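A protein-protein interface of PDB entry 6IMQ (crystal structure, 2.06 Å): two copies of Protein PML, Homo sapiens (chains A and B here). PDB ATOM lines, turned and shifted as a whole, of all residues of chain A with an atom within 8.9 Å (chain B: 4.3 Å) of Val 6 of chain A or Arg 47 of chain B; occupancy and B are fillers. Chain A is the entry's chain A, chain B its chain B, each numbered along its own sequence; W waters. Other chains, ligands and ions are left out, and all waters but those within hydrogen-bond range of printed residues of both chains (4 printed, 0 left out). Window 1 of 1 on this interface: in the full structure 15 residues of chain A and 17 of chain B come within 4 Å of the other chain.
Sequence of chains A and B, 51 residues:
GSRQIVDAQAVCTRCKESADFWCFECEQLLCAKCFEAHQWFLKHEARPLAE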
ATOM      1  N   SER A   2       9.689 -31.267 -41.206  1.00  0.00           N
ATOM      2  CA  SER A   2       8.498 -30.498 -41.541  1.00  0.00           C
ATOM      3  C   SER A   2       8.477 -29.175 -40.774  1.00  0.00           C
ATOM      4  O   SER A   2       9.390 -28.884 -40.000  1.00  0.00           O
ATOM      5  CB  SER A   2       7.238 -31.311 -41.243  1.00  0.00           C
ATOM      6  OG  SER A   2       6.176 -30.909 -42.092  1.00  0.00           O
ATOM      7  N   ARG A   3       7.429 -28.380 -40.985  1.00  0.00           N
ATOM      8  CA  ARG A   3       7.430 -27.004 -40.501  1.00  0.00           C
ATOM      9  C   ARG A   3       7.248 -26.989 -38.990  1.00  0.00           C
ATOM     10  O   ARG A   3       6.314 -27.597 -38.459  1.00  0.00           O
ATOM     11  CB  ARG A   3       6.313 -26.213 -41.178  1.00  0.00           C
ATOM     12  CG  ARG A   3       6.136 -24.789 -40.679  1.00  0.00           C
ATOM     13  CD  ARG A   3       5.041 -24.085 -41.479  1.00  0.00           C
ATOM     14  NE  ARG A   3       3.740 -24.613 -41.071  1.00  0.00           N
ATOM     15  CZ  ARG A   3       2.572 -24.259 -41.596  1.00  0.00           C
ATOM     16  NH1 ARG A   3       2.521 -23.368 -42.575  1.00  0.00           N
ATOM     17  NH2 ARG A   3       1.450 -24.802 -41.139  1.00  0.00           N
ATOM     18  N   GLN A   4       8.141 -26.293 -38.296  1.00  0.00           N
ATOM     19  CA  GLN A   4       8.064 -26.221 -36.846  1.00  0.00           C
ATOM     20  C   GLN A   4       8.843 -25.019 -36.344  1.00  0.00           C
ATOM     21  O   GLN A   4       9.635 -24.415 -37.073  1.00  0.00           O
ATOM     22  CB  GLN A   4       8.562 -27.519 -36.202  1.00  0.00           C
ATOM     23  CG  GLN A   4      10.025 -27.851 -36.409  1.00  0.00           C
ATOM     24  CD  GLN A   4      10.327 -29.318 -36.113  1.00  0.00           C
ATOM     25  OE1 GLN A   4      10.530 -29.699 -34.957  1.00  0.00           O
ATOM     26  NE2 GLN A   4      10.326 -30.149 -37.153  1.00  0.00           N
ATOM     27  N   ILE A   5       8.579 -24.664 -35.093  1.00  0.00           N
ATOM     28  CA  ILE A   5       9.245 -23.558 -34.422  1.00  0.00           C
ATOM     29  C   ILE A   5      10.296 -24.128 -33.484  1.00  0.00           C
ATOM     30  O   ILE A   5      10.048 -25.115 -32.779  1.00  0.00           O
ATOM     31  CB  ILE A   5       8.240 -22.682 -33.651  1.00  0.00           C
ATOM     32  CG1 ILE A   5       7.318 -21.931 -34.617  1.00  0.00           C
ATOM     33  CG2 ILE A   5       8.981 -21.702 -32.747  1.00  0.00           C
ATOM     34  CD1 ILE A   5       6.391 -22.814 -35.416  1.00  0.00           C
ATOM     35  N   VAL A   6      11.468 -23.510 -33.472  1.00  0.00           N
ATOM     36  CA  VAL A   6      12.517 -23.848 -32.521  1.00  0.00           C
ATOM     37  C   VAL A   6      12.839 -22.588 -31.733  1.00  0.00           C
ATOM     38  O   VAL A   6      12.647 -21.462 -32.212  1.00  0.00           O
ATOM     39  CB  VAL A   6      13.770 -24.420 -33.216  1.00  0.00           C
ATOM     40  CG1 VAL A   6      13.422 -25.731 -33.917  1.00  0.00           C
ATOM     41  CG2 VAL A   6      14.340 -23.420 -34.180  1.00  0.00           C
ATOM     42  N   ASP A   7      13.282 -22.781 -30.497  1.00  0.00           N
ATOM     43  CA  ASP A   7      13.584 -21.679 -29.603  1.00  0.00           C
ATOM     44  C   ASP A   7      15.066 -21.680 -29.252  1.00  0.00           C
ATOM     45  O   ASP A   7      15.768 -22.683 -29.434  1.00  0.00           O
ATOM     46  CB  ASP A   7      12.732 -21.772 -28.333  1.00  0.00           C
ATOM     47  CG  ASP A   7      12.583 -20.438 -27.625  1.00  0.00           C
ATOM     48  OD1 ASP A   7      13.572 -19.677 -27.539  1.00  0.00           O
ATOM     49  OD2 ASP A   7      11.460 -20.151 -27.157  1.00  0.00           O
ATOM     50  N   ALA A   8      15.536 -20.537 -28.744  1.00  0.00           N
ATOM     51  CA  ALA A   8      16.914 -20.465 -28.282  1.00  0.00           C
ATOM     52  C   ALA A   8      17.109 -21.233 -26.986  1.00  0.00           C
ATOM     53  O   ALA A   8      18.233 -21.658 -26.689  1.00  0.00           O
ATOM     54  CB  ALA A   8      17.318 -19.007 -28.073  1.00  0.00           C
ATOM     55  N   GLN A   9      16.032 -21.463 -26.243  1.00  0.00           N
ATOM     56  CA  GLN A   9      16.063 -22.186 -24.986  1.00  0.00           C
ATOM     57  C   GLN A   9      15.113 -23.368 -25.051  1.00  0.00           C
ATOM     58  O   GLN A   9      14.042 -23.288 -25.660  1.00  0.00           O
ATOM     59  CB  GLN A   9      15.691 -21.264 -23.825  1.00  0.00           C
ATOM     60  CG  GLN A   9      16.873 -20.955 -22.929  1.00  0.00           C
ATOM     61  CD  GLN A   9      16.667 -19.737 -22.057  1.00  0.00           C
ATOM     62  OE1 GLN A   9      15.539 -19.300 -21.826  1.00  0.00           O
ATOM     63  NE2 GLN A   9      17.765 -19.183 -21.556  1.00  0.00           N
ATOM     64  N   ALA A  10      15.535 -24.469 -24.449  1.00  0.00           N
ATOM     65  CA  ALA A  10      14.740 -25.686 -24.414  1.00  0.00           C
ATOM     66  C   ALA A  10      13.773 -25.589 -23.241  1.00  0.00           C
ATOM     67  O   ALA A  10      14.203 -25.519 -22.083  1.00  0.00           O
ATOM     68  CB  ALA A  10      15.637 -26.912 -24.273  1.00  0.00           C
ATOM     69  N   VAL A  11      12.475 -25.571 -23.538  1.00  0.00           N
ATOM     70  CA  VAL A  11      11.469 -25.473 -22.490  1.00  0.00           C
ATOM     71  C   VAL A  11      10.406 -26.545 -22.666  1.00  0.00           C
ATOM     72  O   VAL A  11      10.033 -26.918 -23.781  1.00  0.00           O
ATOM     73  CB  VAL A  11      10.819 -24.072 -22.445  1.00  0.00           C
ATOM     74  CG1 VAL A  11      11.846 -23.027 -22.008  1.00  0.00           C
ATOM     75  CG2 VAL A  11      10.235 -23.714 -23.796  1.00  0.00           C
ATOM     76  N   THR A  13       7.276 -28.638 -23.192  1.00  0.00           N
ATOM     77  CA  THR A  13       6.099 -28.418 -24.019  1.00  0.00           C
ATOM     78  C   THR A  13       4.836 -28.258 -23.185  1.00  0.00           C
ATOM     79  O   THR A  13       3.901 -27.571 -23.607  1.00  0.00           O
ATOM     80  CB  THR A  13       5.940 -29.578 -24.999  1.00  0.00           C
ATOM     81  OG1 THR A  13       7.178 -29.801 -25.687  1.00  0.00           O
ATOM     82  CG2 THR A  13       4.855 -29.262 -26.016  1.00  0.00           C
ATOM     83  N   ALA A  19      13.588 -27.515 -20.040  1.00  0.00           N
ATOM     84  CA  ALA A  19      13.406 -28.891 -20.483  1.00  0.00           C
ATOM     85  C   ALA A  19      14.631 -29.756 -20.209  1.00  0.00           C
ATOM     86  O   ALA A  19      15.766 -29.274 -20.171  1.00  0.00           O
ATOM     87  CB  ALA A  19      13.101 -28.948 -21.982  1.00  0.00           C
ATOM     88  N   PHE A  21      14.317 -33.558 -21.298  1.00  0.00           N
ATOM     89  CA  PHE A  21      14.183 -34.780 -22.074  1.00  0.00           C
ATOM     90  C   PHE A  21      13.476 -34.498 -23.396  1.00  0.00           C
ATOM     91  O   PHE A  21      12.748 -33.514 -23.538  1.00  0.00           O
ATOM     92  CB  PHE A  21      13.379 -35.866 -21.332  1.00  0.00           C
ATOM     93  CG  PHE A  21      14.031 -36.374 -20.090  1.00  0.00           C
ATOM     94  CD1 PHE A  21      14.797 -37.524 -20.118  1.00  0.00           C
ATOM     95  CD2 PHE A  21      13.855 -35.720 -18.887  1.00  0.00           C
ATOM     96  CE1 PHE A  21      15.393 -38.010 -18.968  1.00  0.00           C
ATOM     97  CE2 PHE A  21      14.454 -36.193 -17.731  1.00  0.00           C
ATOM     98  CZ  PHE A  21      15.221 -37.339 -17.772  1.00  0.00           C
ATOM     99  N   TRP A  22      13.697 -35.389 -24.364  1.00  0.00           N
ATOM    100  CA  TRP A  22      12.956 -35.417 -25.621  1.00  0.00           C
ATOM    101  C   TRP A  22      12.369 -36.804 -25.822  1.00  0.00           C
ATOM    102  O   TRP A  22      13.108 -37.790 -25.793  1.00  0.00           O
ATOM    103  CB  TRP A  22      13.865 -35.088 -26.806  1.00  0.00           C
ATOM    104  CG  TRP A  22      13.234 -35.294 -28.146  1.00  0.00           C
ATOM    105  CD1 TRP A  22      13.400 -36.367 -28.971  1.00  0.00           C
ATOM    106  CD2 TRP A  22      12.342 -34.396 -28.821  1.00  0.00           C
ATOM    107  NE1 TRP A  22      12.665 -36.190 -30.124  1.00  0.00           N
ATOM    108  CE2 TRP A  22      12.006 -34.993 -30.052  1.00  0.00           C
ATOM    109  CE3 TRP A  22      11.789 -33.155 -28.497  1.00  0.00           C
ATOM    110  CZ2 TRP A  22      11.146 -34.382 -30.962  1.00  0.00           C
ATOM    111  CZ3 TRP A  22      10.939 -32.553 -29.404  1.00  0.00           C
ATOM    112  CH2 TRP A  22      10.625 -33.166 -30.621  1.00  0.00           C
ATOM    113  N   CYS A  23      11.065 -36.886 -26.070  1.00  0.00           N
ATOM    114  CA  CYS A  23      10.435 -38.172 -26.348  1.00  0.00           C
ATOM    115  C   CYS A  23      10.193 -38.316 -27.847  1.00  0.00           C
ATOM    116  O   CYS A  23       9.470 -37.514 -28.445  1.00  0.00           O
ATOM    117  CB  CYS A  23       9.110 -38.341 -25.609  1.00  0.00           C
ATOM    118  SG  CYS A  23       8.260 -39.857 -26.157  1.00  0.00           S
ATOM    119  N   PHE A  24      10.748 -39.376 -28.439  1.00  0.00           N
ATOM    120  CA  PHE A  24      10.660 -39.538 -29.884  1.00  0.00           C
ATOM    121  C   PHE A  24       9.252 -39.856 -30.357  1.00  0.00           C
ATOM    122  O   PHE A  24       8.909 -39.564 -31.508  1.00  0.00           O
ATOM    123  CB  PHE A  24      11.604 -40.641 -30.345  1.00  0.00           C
ATOM    124  CG  PHE A  24      13.031 -40.244 -30.338  1.00  0.00           C
ATOM    125  CD1 PHE A  24      13.541 -39.474 -31.363  1.00  0.00           C
ATOM    126  CD2 PHE A  24      13.864 -40.615 -29.299  1.00  0.00           C
ATOM    127  CE1 PHE A  24      14.861 -39.100 -31.369  1.00  0.00           C
ATOM    128  CE2 PHE A  24      15.183 -40.236 -29.296  1.00  0.00           C
ATOM    129  CZ  PHE A  24      15.682 -39.473 -30.330  1.00  0.00           C
ATOM    130  N   GLU A  27       7.207 -36.662 -29.500  1.00  0.00           N
ATOM    131  CA  GLU A  27       7.835 -35.520 -30.175  1.00  0.00           C
ATOM    132  C   GLU A  27       7.643 -34.261 -29.332  1.00  0.00           C
ATOM    133  O   GLU A  27       7.042 -33.267 -29.752  1.00  0.00           O
ATOM    134  CB  GLU A  27       7.280 -35.323 -31.592  1.00  0.00           C
ATOM    135  CG  GLU A  27       7.161 -36.602 -32.410  1.00  0.00           C
ATOM    136  CD  GLU A  27       8.089 -36.636 -33.619  1.00  0.00           C
ATOM    137  OE1 GLU A  27       7.702 -36.142 -34.701  1.00  0.00           O
ATOM    138  OE2 GLU A  27       9.210 -37.172 -33.483  1.00  0.00           O
ATOM    139  N   GLN A  28       8.153 -34.334 -28.106  1.00  0.00           N
ATOM    140  CA  GLN A  28       7.903 -33.299 -27.121  1.00  0.00           C
ATOM    141  C   GLN A  28       9.139 -33.111 -26.262  1.00  0.00           C
ATOM    142  O   GLN A  28       9.811 -34.089 -25.921  1.00  0.00           O
ATOM    143  CB  GLN A  28       6.769 -33.657 -26.166  1.00  0.00           C
ATOM    144  CG  GLN A  28       5.391 -33.330 -26.586  1.00  0.00           C
ATOM    145  CD  GLN A  28       4.351 -33.797 -25.566  1.00  0.00           C
ATOM    146  OE1 GLN A  28       4.514 -33.544 -24.365  1.00  0.00           O
ATOM    147  NE2 GLN A  28       3.448 -34.672 -25.992  1.00  0.00           N
ATOM    148  N   LEU A  29       9.377 -31.872 -25.856  1.00  0.00           N
ATOM    149  CA  LEU A  29      10.333 -31.551 -24.813  1.00  0.00           C
ATOM    150  C   LEU A  29       9.631 -31.556 -23.463  1.00  0.00           C
ATOM    151  O   LEU A  29       8.569 -30.945 -23.314  1.00  0.00           O
ATOM    152  CB  LEU A  29      10.930 -30.175 -25.067  1.00  0.00           C
ATOM    153  CG  LEU A  29      11.750 -30.006 -26.340  1.00  0.00           C
ATOM    154  CD1 LEU A  29      11.858 -28.537 -26.655  1.00  0.00           C
ATOM    155  CD2 LEU A  29      13.075 -30.666 -26.120  1.00  0.00           C
ATOM    156  N   LEU A  30      10.246 -32.200 -22.471  1.00  0.00           N
ATOM    157  CA  LEU A  30       9.674 -32.299 -21.138  1.00  0.00           C
ATOM    158  C   LEU A  30      10.707 -31.979 -20.065  1.00  0.00           C
ATOM    159  O   LEU A  30      11.867 -32.388 -20.159  1.00  0.00           O
ATOM    160  CB  LEU A  30       9.109 -33.705 -20.921  1.00  0.00           C
ATOM    161  CG  LEU A  30       8.019 -34.071 -21.930  1.00  0.00           C
ATOM    162  CD1 LEU A  30       7.698 -35.556 -21.911  1.00  0.00           C
ATOM    163  CD2 LEU A  30       6.750 -33.247 -21.670  1.00  0.00           C
ATOM    164  N   ARG A  47      15.280 -39.601 -24.610  1.00  0.00           N
ATOM    165  CA  ARG A  47      16.670 -39.351 -24.254  1.00  0.00           C
ATOM    166  C   ARG A  47      16.753 -38.033 -23.520  1.00  0.00           C
ATOM    167  O   ARG A  47      15.898 -37.155 -23.729  1.00  0.00           O
ATOM    168  CB  ARG A  47      17.559 -39.285 -25.506  1.00  0.00           C
ATOM    169  CG  ARG A  47      16.963 -38.309 -26.516  1.00  0.00           C
ATOM    170  CD  ARG A  47      17.786 -38.150 -27.774  1.00  0.00           C
ATOM    171  NE  ARG A  47      19.155 -37.700 -27.570  1.00  0.00           N
ATOM    172  CZ  ARG A  47      19.586 -36.464 -27.793  1.00  0.00           C
ATOM    173  NH1 ARG A  47      18.757 -35.518 -28.215  1.00  0.00           N
ATOM    174  NH2 ARG A  47      20.862 -36.182 -27.594  1.00  0.00           N
ATOM    175  N   PRO A  48      17.745 -37.847 -22.655  1.00  0.00           N
ATOM    176  CA  PRO A  48      18.016 -36.514 -22.113  1.00  0.00           C
ATOM    177  C   PRO A  48      18.506 -35.595 -23.222  1.00  0.00           C
ATOM    178  O   PRO A  48      19.042 -36.031 -24.244  1.00  0.00           O
ATOM    179  CB  PRO A  48      19.107 -36.746 -21.061  1.00  0.00           C
ATOM    180  CG  PRO A  48      19.268 -38.264 -20.951  1.00  0.00           C
ATOM    181  CD  PRO A  48      18.771 -38.832 -22.254  1.00  0.00           C
ATOM    182  N   LEU A  49      18.309 -34.296 -23.006  1.00  0.00           N
ATOM    183  CA  LEU A  49      18.677 -33.326 -24.026  1.00  0.00           C
ATOM    184  C   LEU A  49      20.182 -33.184 -24.189  1.00  0.00           C
ATOM    185  O   LEU A  49      20.651 -32.862 -25.287  1.00  0.00           O
ATOM    186  CB  LEU A  49      18.095 -31.969 -23.660  1.00  0.00           C
ATOM    187  CG  LEU A  49      16.637 -31.660 -23.957  1.00  0.00           C
ATOM    188  CD1 LEU A  49      16.377 -30.215 -23.592  1.00  0.00           C
ATOM    189  CD2 LEU A  49      16.385 -31.898 -25.428  1.00  0.00           C
ATOM    190  N   ALA A  50      20.949 -33.448 -23.138  1.00  0.00           N
ATOM    191  CA  ALA A  50      22.403 -33.420 -23.220  1.00  0.00           C
ATOM    192  C   ALA A  50      22.950 -34.832 -23.045  1.00  0.00           C
ATOM    193  O   ALA A  50      22.589 -35.744 -23.788  1.00  0.00           O
ATOM    194  CB  ALA A  50      22.975 -32.478 -22.177  1.00  0.00           C
ATOM    195  N   SER B   2      14.433 -15.753 -28.661  1.00  0.00           N
ATOM    196  CA  SER B   2      14.332 -15.763 -30.112  1.00  0.00           C
ATOM    197  C   SER B   2      13.820 -17.113 -30.599  1.00  0.00           C
ATOM    198  O   SER B   2      14.542 -18.112 -30.580  1.00  0.00           O
ATOM    199  CB  SER B   2      15.685 -15.444 -30.756  1.00  0.00           C
ATOM    200  OG  SER B   2      16.519 -16.580 -30.835  1.00  0.00           O
ATOM    201  N   ARG B   3      12.555 -17.145 -31.005  1.00  0.00           N
ATOM    202  CA  ARG B   3      12.024 -18.310 -31.691  1.00  0.00           C
ATOM    203  C   ARG B   3      12.408 -18.248 -33.164  1.00  0.00           C
ATOM    204  O   ARG B   3      12.738 -17.187 -33.706  1.00  0.00           O
ATOM    205  CB  ARG B   3      10.505 -18.390 -31.563  1.00  0.00           C
ATOM    206  CG  ARG B   3       9.925 -17.869 -30.256  1.00  0.00           C
ATOM    207  CD  ARG B   3       8.446 -18.261 -30.148  1.00  0.00           C
ATOM    208  NE  ARG B   3       8.280 -19.615 -29.622  1.00  0.00           N
ATOM    209  CZ  ARG B   3       7.286 -20.440 -29.936  1.00  0.00           C
ATOM    210  NH1 ARG B   3       6.350 -20.075 -30.799  1.00  0.00           N
ATOM    211  NH2 ARG B   3       7.243 -21.644 -29.389  1.00  0.00           N
ATOM    212  N   GLN B   4      12.342 -19.399 -33.822  1.00  0.00           N
ATOM    213  CA  GLN B   4      12.788 -19.491 -35.201  1.00  0.00           C
ATOM    214  C   GLN B   4      11.911 -20.480 -35.939  1.00  0.00           C
ATOM    215  O   GLN B   4      11.565 -21.535 -35.399  1.00  0.00           O
ATOM    216  CB  GLN B   4      14.253 -19.919 -35.261  1.00  0.00           C
ATOM    217  CG  GLN B   4      15.001 -19.423 -36.457  1.00  0.00           C
ATOM    218  CD  GLN B   4      16.470 -19.785 -36.383  1.00  0.00           C
ATOM    219  OE1 GLN B   4      16.952 -20.639 -37.124  1.00  0.00           O
ATOM    220  NE2 GLN B   4      17.187 -19.145 -35.476  1.00  0.00           N
ATOM    221  N   VAL B   6      11.533 -23.214 -38.735  1.00  0.00           N
ATOM    222  CA  VAL B   6      12.360 -24.182 -39.443  1.00  0.00           C
ATOM    223  C   VAL B   6      11.467 -24.797 -40.513  1.00  0.00           C
ATOM    224  O   VAL B   6      10.574 -25.601 -40.219  1.00  0.00           O
ATOM    225  CB  VAL B   6      12.967 -25.235 -38.516  1.00  0.00           C
ATOM    226  CG1 VAL B   6      13.349 -26.483 -39.267  1.00  0.00           C
ATOM    227  CG2 VAL B   6      14.200 -24.612 -37.836  1.00  0.00           C
ATOM    228  N   PHE B  21      18.478 -32.184 -36.536  1.00  0.00           N
ATOM    229  CA  PHE B  21      18.715 -31.801 -35.163  1.00  0.00           C
ATOM    230  C   PHE B  21      18.843 -30.294 -35.076  1.00  0.00           C
ATOM    231  O   PHE B  21      19.185 -29.609 -36.041  1.00  0.00           O
ATOM    232  CB  PHE B  21      19.964 -32.479 -34.604  1.00  0.00           C
ATOM    233  CG  PHE B  21      19.834 -33.952 -34.509  1.00  0.00           C
ATOM    234  CD1 PHE B  21      20.073 -34.758 -35.606  1.00  0.00           C
ATOM    235  CD2 PHE B  21      19.439 -34.535 -33.321  1.00  0.00           C
ATOM    236  CE1 PHE B  21      19.937 -36.125 -35.514  1.00  0.00           C
ATOM    237  CE2 PHE B  21      19.300 -35.897 -33.216  1.00  0.00           C
ATOM    238  CZ  PHE B  21      19.545 -36.700 -34.314  1.00  0.00           C
ATOM    239  N   TRP B  22      18.501 -29.793 -33.901  1.00  0.00           N
ATOM    240  CA  TRP B  22      18.623 -28.388 -33.552  1.00  0.00           C
ATOM    241  C   TRP B  22      19.456 -28.330 -32.287  1.00  0.00           C
ATOM    242  O   TRP B  22      19.155 -29.026 -31.309  1.00  0.00           O
ATOM    243  CB  TRP B  22      17.259 -27.744 -33.337  1.00  0.00           C
ATOM    244  CG  TRP B  22      17.305 -26.364 -32.740  1.00  0.00           C
ATOM    245  CD1 TRP B  22      16.998 -26.023 -31.458  1.00  0.00           C
ATOM    246  CD2 TRP B  22      17.658 -25.144 -33.405  1.00  0.00           C
ATOM    247  NE1 TRP B  22      17.133 -24.667 -31.279  1.00  0.00           N
ATOM    248  CE2 TRP B  22      17.536 -24.103 -32.461  1.00  0.00           C
ATOM    249  CE3 TRP B  22      18.060 -24.830 -34.705  1.00  0.00           C
ATOM    250  CZ2 TRP B  22      17.811 -22.776 -32.775  1.00  0.00           C
ATOM    251  CZ3 TRP B  22      18.329 -23.510 -35.015  1.00  0.00           C
ATOM    252  CH2 TRP B  22      18.201 -22.499 -34.056  1.00  0.00           C
ATOM    253  N   PHE B  24      20.568 -26.106 -29.171  1.00  0.00           N
ATOM    254  CA  PHE B  24      20.101 -24.927 -28.456  1.00  0.00           C
ATOM    255  C   PHE B  24      21.230 -23.950 -28.141  1.00  0.00           C
ATOM    256  O   PHE B  24      20.981 -22.745 -28.028  1.00  0.00           O
ATOM    257  CB  PHE B  24      19.394 -25.354 -27.169  1.00  0.00           C
ATOM    258  CG  PHE B  24      18.098 -26.058 -27.402  1.00  0.00           C
ATOM    259  CD1 PHE B  24      17.004 -25.356 -27.865  1.00  0.00           C
ATOM    260  CD2 PHE B  24      17.964 -27.417 -27.165  1.00  0.00           C
ATOM    261  CE1 PHE B  24      15.802 -25.982 -28.089  1.00  0.00           C
ATOM    262  CE2 PHE B  24      16.760 -28.052 -27.383  1.00  0.00           C
ATOM    263  CZ  PHE B  24      15.675 -27.330 -27.850  1.00  0.00           C
ATOM    264  N   ALA B  46      20.662 -30.223 -27.187  1.00  0.00           N
ATOM    265  CA  ALA B  46      20.171 -30.243 -28.557  1.00  0.00           C
ATOM    266  C   ALA B  46      19.007 -31.208 -28.612  1.00  0.00           C
ATOM    267  O   ALA B  46      18.809 -32.028 -27.708  1.00  0.00           O
ATOM    268  CB  ALA B  46      21.266 -30.646 -29.551  1.00  0.00           C
ATOM    269  N   ARG B  47      18.247 -31.125 -29.692  1.00  0.00           N
ATOM    270  CA  ARG B  47      17.091 -31.986 -29.798  1.00  0.00           C
ATOM    271  C   ARG B  47      16.851 -32.446 -31.224  1.00  0.00           C
ATOM    272  O   ARG B  47      17.178 -31.734 -32.183  1.00  0.00           O
ATOM    273  CB  ARG B  47      15.834 -31.270 -29.290  1.00  0.00           C
ATOM    274  CG  ARG B  47      15.310 -30.206 -30.225  1.00  0.00           C
ATOM    275  CD  ARG B  47      13.815 -30.228 -30.065  1.00  0.00           C
ATOM    276  NE  ARG B  47      13.102 -29.051 -30.510  1.00  0.00           N
ATOM    277  CZ  ARG B  47      12.228 -29.068 -31.508  1.00  0.00           C
ATOM    278  NH1 ARG B  47      11.987 -30.193 -32.171  1.00  0.00           N
ATOM    279  NH2 ARG B  47      11.595 -27.959 -31.841  1.00  0.00           N
ATOM    280  N   PRO B  48      16.259 -33.626 -31.386  1.00  0.00           N
ATOM    281  CA  PRO B  48      15.717 -33.998 -32.694  1.00  0.00           C
ATOM    282  C   PRO B  48      14.654 -33.000 -33.116  1.00  0.00           C
ATOM    283  O   PRO B  48      13.986 -32.383 -32.287  1.00  0.00           O
ATOM    284  CB  PRO B  48      15.122 -35.393 -32.459  1.00  0.00           C
ATOM    285  CG  PRO B  48      15.810 -35.899 -31.194  1.00  0.00           C
ATOM    286  CD  PRO B  48      16.011 -34.659 -30.362  1.00  0.00           C
ATOM    287  N   LEU B  49      14.520 -32.829 -34.423  1.00  0.00           N
ATOM    288  CA  LEU B  49      13.411 -32.074 -34.977  1.00  0.00           C
ATOM    289  C   LEU B  49      12.209 -33.001 -35.100  1.00  0.00           C
ATOM    290  O   LEU B  49      12.358 -34.193 -35.382  1.00  0.00           O
ATOM    291  CB  LEU B  49      13.776 -31.486 -36.336  1.00  0.00           C
ATOM    292  CG  LEU B  49      14.821 -30.374 -36.302  1.00  0.00           C
ATOM    293  CD1 LEU B  49      15.203 -30.094 -37.769  1.00  0.00           C
ATOM    294  CD2 LEU B  49      14.370 -29.119 -35.631  1.00  0.00           C
ATOM    295  N   ALA B  50      11.020 -32.456 -34.858  1.00  0.00           N
ATOM    296  CA  ALA B  50       9.809 -33.224 -35.105  1.00  0.00           C
ATOM    297  C   ALA B  50       9.805 -33.681 -36.559  1.00  0.00           C
ATOM    298  O   ALA B  50      10.226 -32.947 -37.457  1.00  0.00           O
ATOM    299  CB  ALA B  50       8.568 -32.388 -34.795  1.00  0.00           C
HETATM  300  O   HOH W   1      20.852 -20.194 -27.078  1.00  0.00           O
HETATM  301  O   HOH W   2      20.777 -22.213 -24.861  1.00  0.00           O
HETATM  302  O   HOH W   3       9.685 -22.148 -26.960  1.00  0.00           O
HETATM  303  O   HOH W   4      22.683 -33.022 -26.946  1.00  0.00           O
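The side-chain amide oxygen (OE1) of Gln 4 of chain A lies within hydrogen-bond range of the backbone NH (N) of Ala 50 of chain B (2.8 Å).
N of Gln 4 of chain B is in hydrogen-bond range of O of Val 6 of chain A, at 2.6 Å.
The backbone carbonyl oxygen of Phe 24 of chain B sits close to the backbone carbonyl oxygen of Ala 8 of chain A (3.2 Å).
O of Ile 5 of chain A is in hydrogen-bond range of NH2 of Arg 47 of chain B (3.4 Å).
The backbone carbonyl oxygen (O) of Ser 2 of chain A lies close to the backbone carbonyl oxygen (O) of Val 6 of chain B.
The backbone carbonyl oxygen of Leu 49 of chain A is in hydrogen-bond range of the backbone NH of Ala 46 of chain B (3.3 Å).
The side-chain amide oxygen (OE1) of Gln 4 of chain A sits at hydrogen-bond distance from the guanidinium group (NH1) of Arg 47 of chain B, 3.2 Å away.
The backbone NH of Ala 8 of chain A is in hydrogen-bond range of the backbone carbonyl oxygen of Ser 2 of chain B (3.2 Å).
N of Val 6 of chain B lies within hydrogen-bond range of O of Gln 4 of chain A (2.8 Å).
The indole nitrogen (NE1) of Trp 22 of chain B sits at hydrogen-bond distance from the backbone carbonyl oxygen (O) of Asp 7 of chain A (3.0 Å).
O of Ala 10 of chain A lies within hydrogen-bond range of N of Ala 19 of chain A, at 2.9 Å.
N of Gln 9 of chain A sits close to OD1 of Asp 7 of chain A.
Of the printed residues of chain B, Gln 4 of chain A touches Gln 4 (3.8 Å), Val 6 (2.8 Å), Arg 47 (3.2 Å), Leu 49 (3.7 Å) and Ala 50 (2.8 Å).
Val 6 of chain A touches six residues of chain B.
Of chain A, only Val 6 and Asp 7 come within 4 Å of Trp 22 of chain B.
Of the printed residues of chain A, Ala 46 of chain B touches Arg 47 (3.5 Å) and Leu 49 (3.2 Å).
The nearest residue of chain B that does not touch Val 6 of chain A is Ser 2 of chain B (4.2 Å).
The nearest residue of chain A that does not touch Arg 47 of chain B is Leu 29 of chain A (4.04 Å).
Of the 12 printed residues of chain B, 11 touch a printed residue of chain A.
Hydrophobic or aromatic side chains of chain B within 4 Å of the printed part of chain A: Val 6, Trp 22, Phe 24, Pro 48, Leu 49 and Ala 50.
Among the printed residues, no Asp or Glu carboxylate lies within 4 Å of a Lys or Arg side-chain nitrogen of the other chain.
Trp 22 of chain A touches Arg 47 of chain B, but with the chains exchanged Arg 47 of chain A does not touch Trp 22 of chain B (7.2 Å).
Water W4 lies within hydrogen-bond range of O of Leu 49 of chain A (2.6 Å) and N of Ala 46 of chain B (3.5 Å).
Water W3 bridges the side-chain carboxylate of Asp 7 of chain A (2.7 Å) and the guanidinium group of Arg 3 of chain B (3.5 Å).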
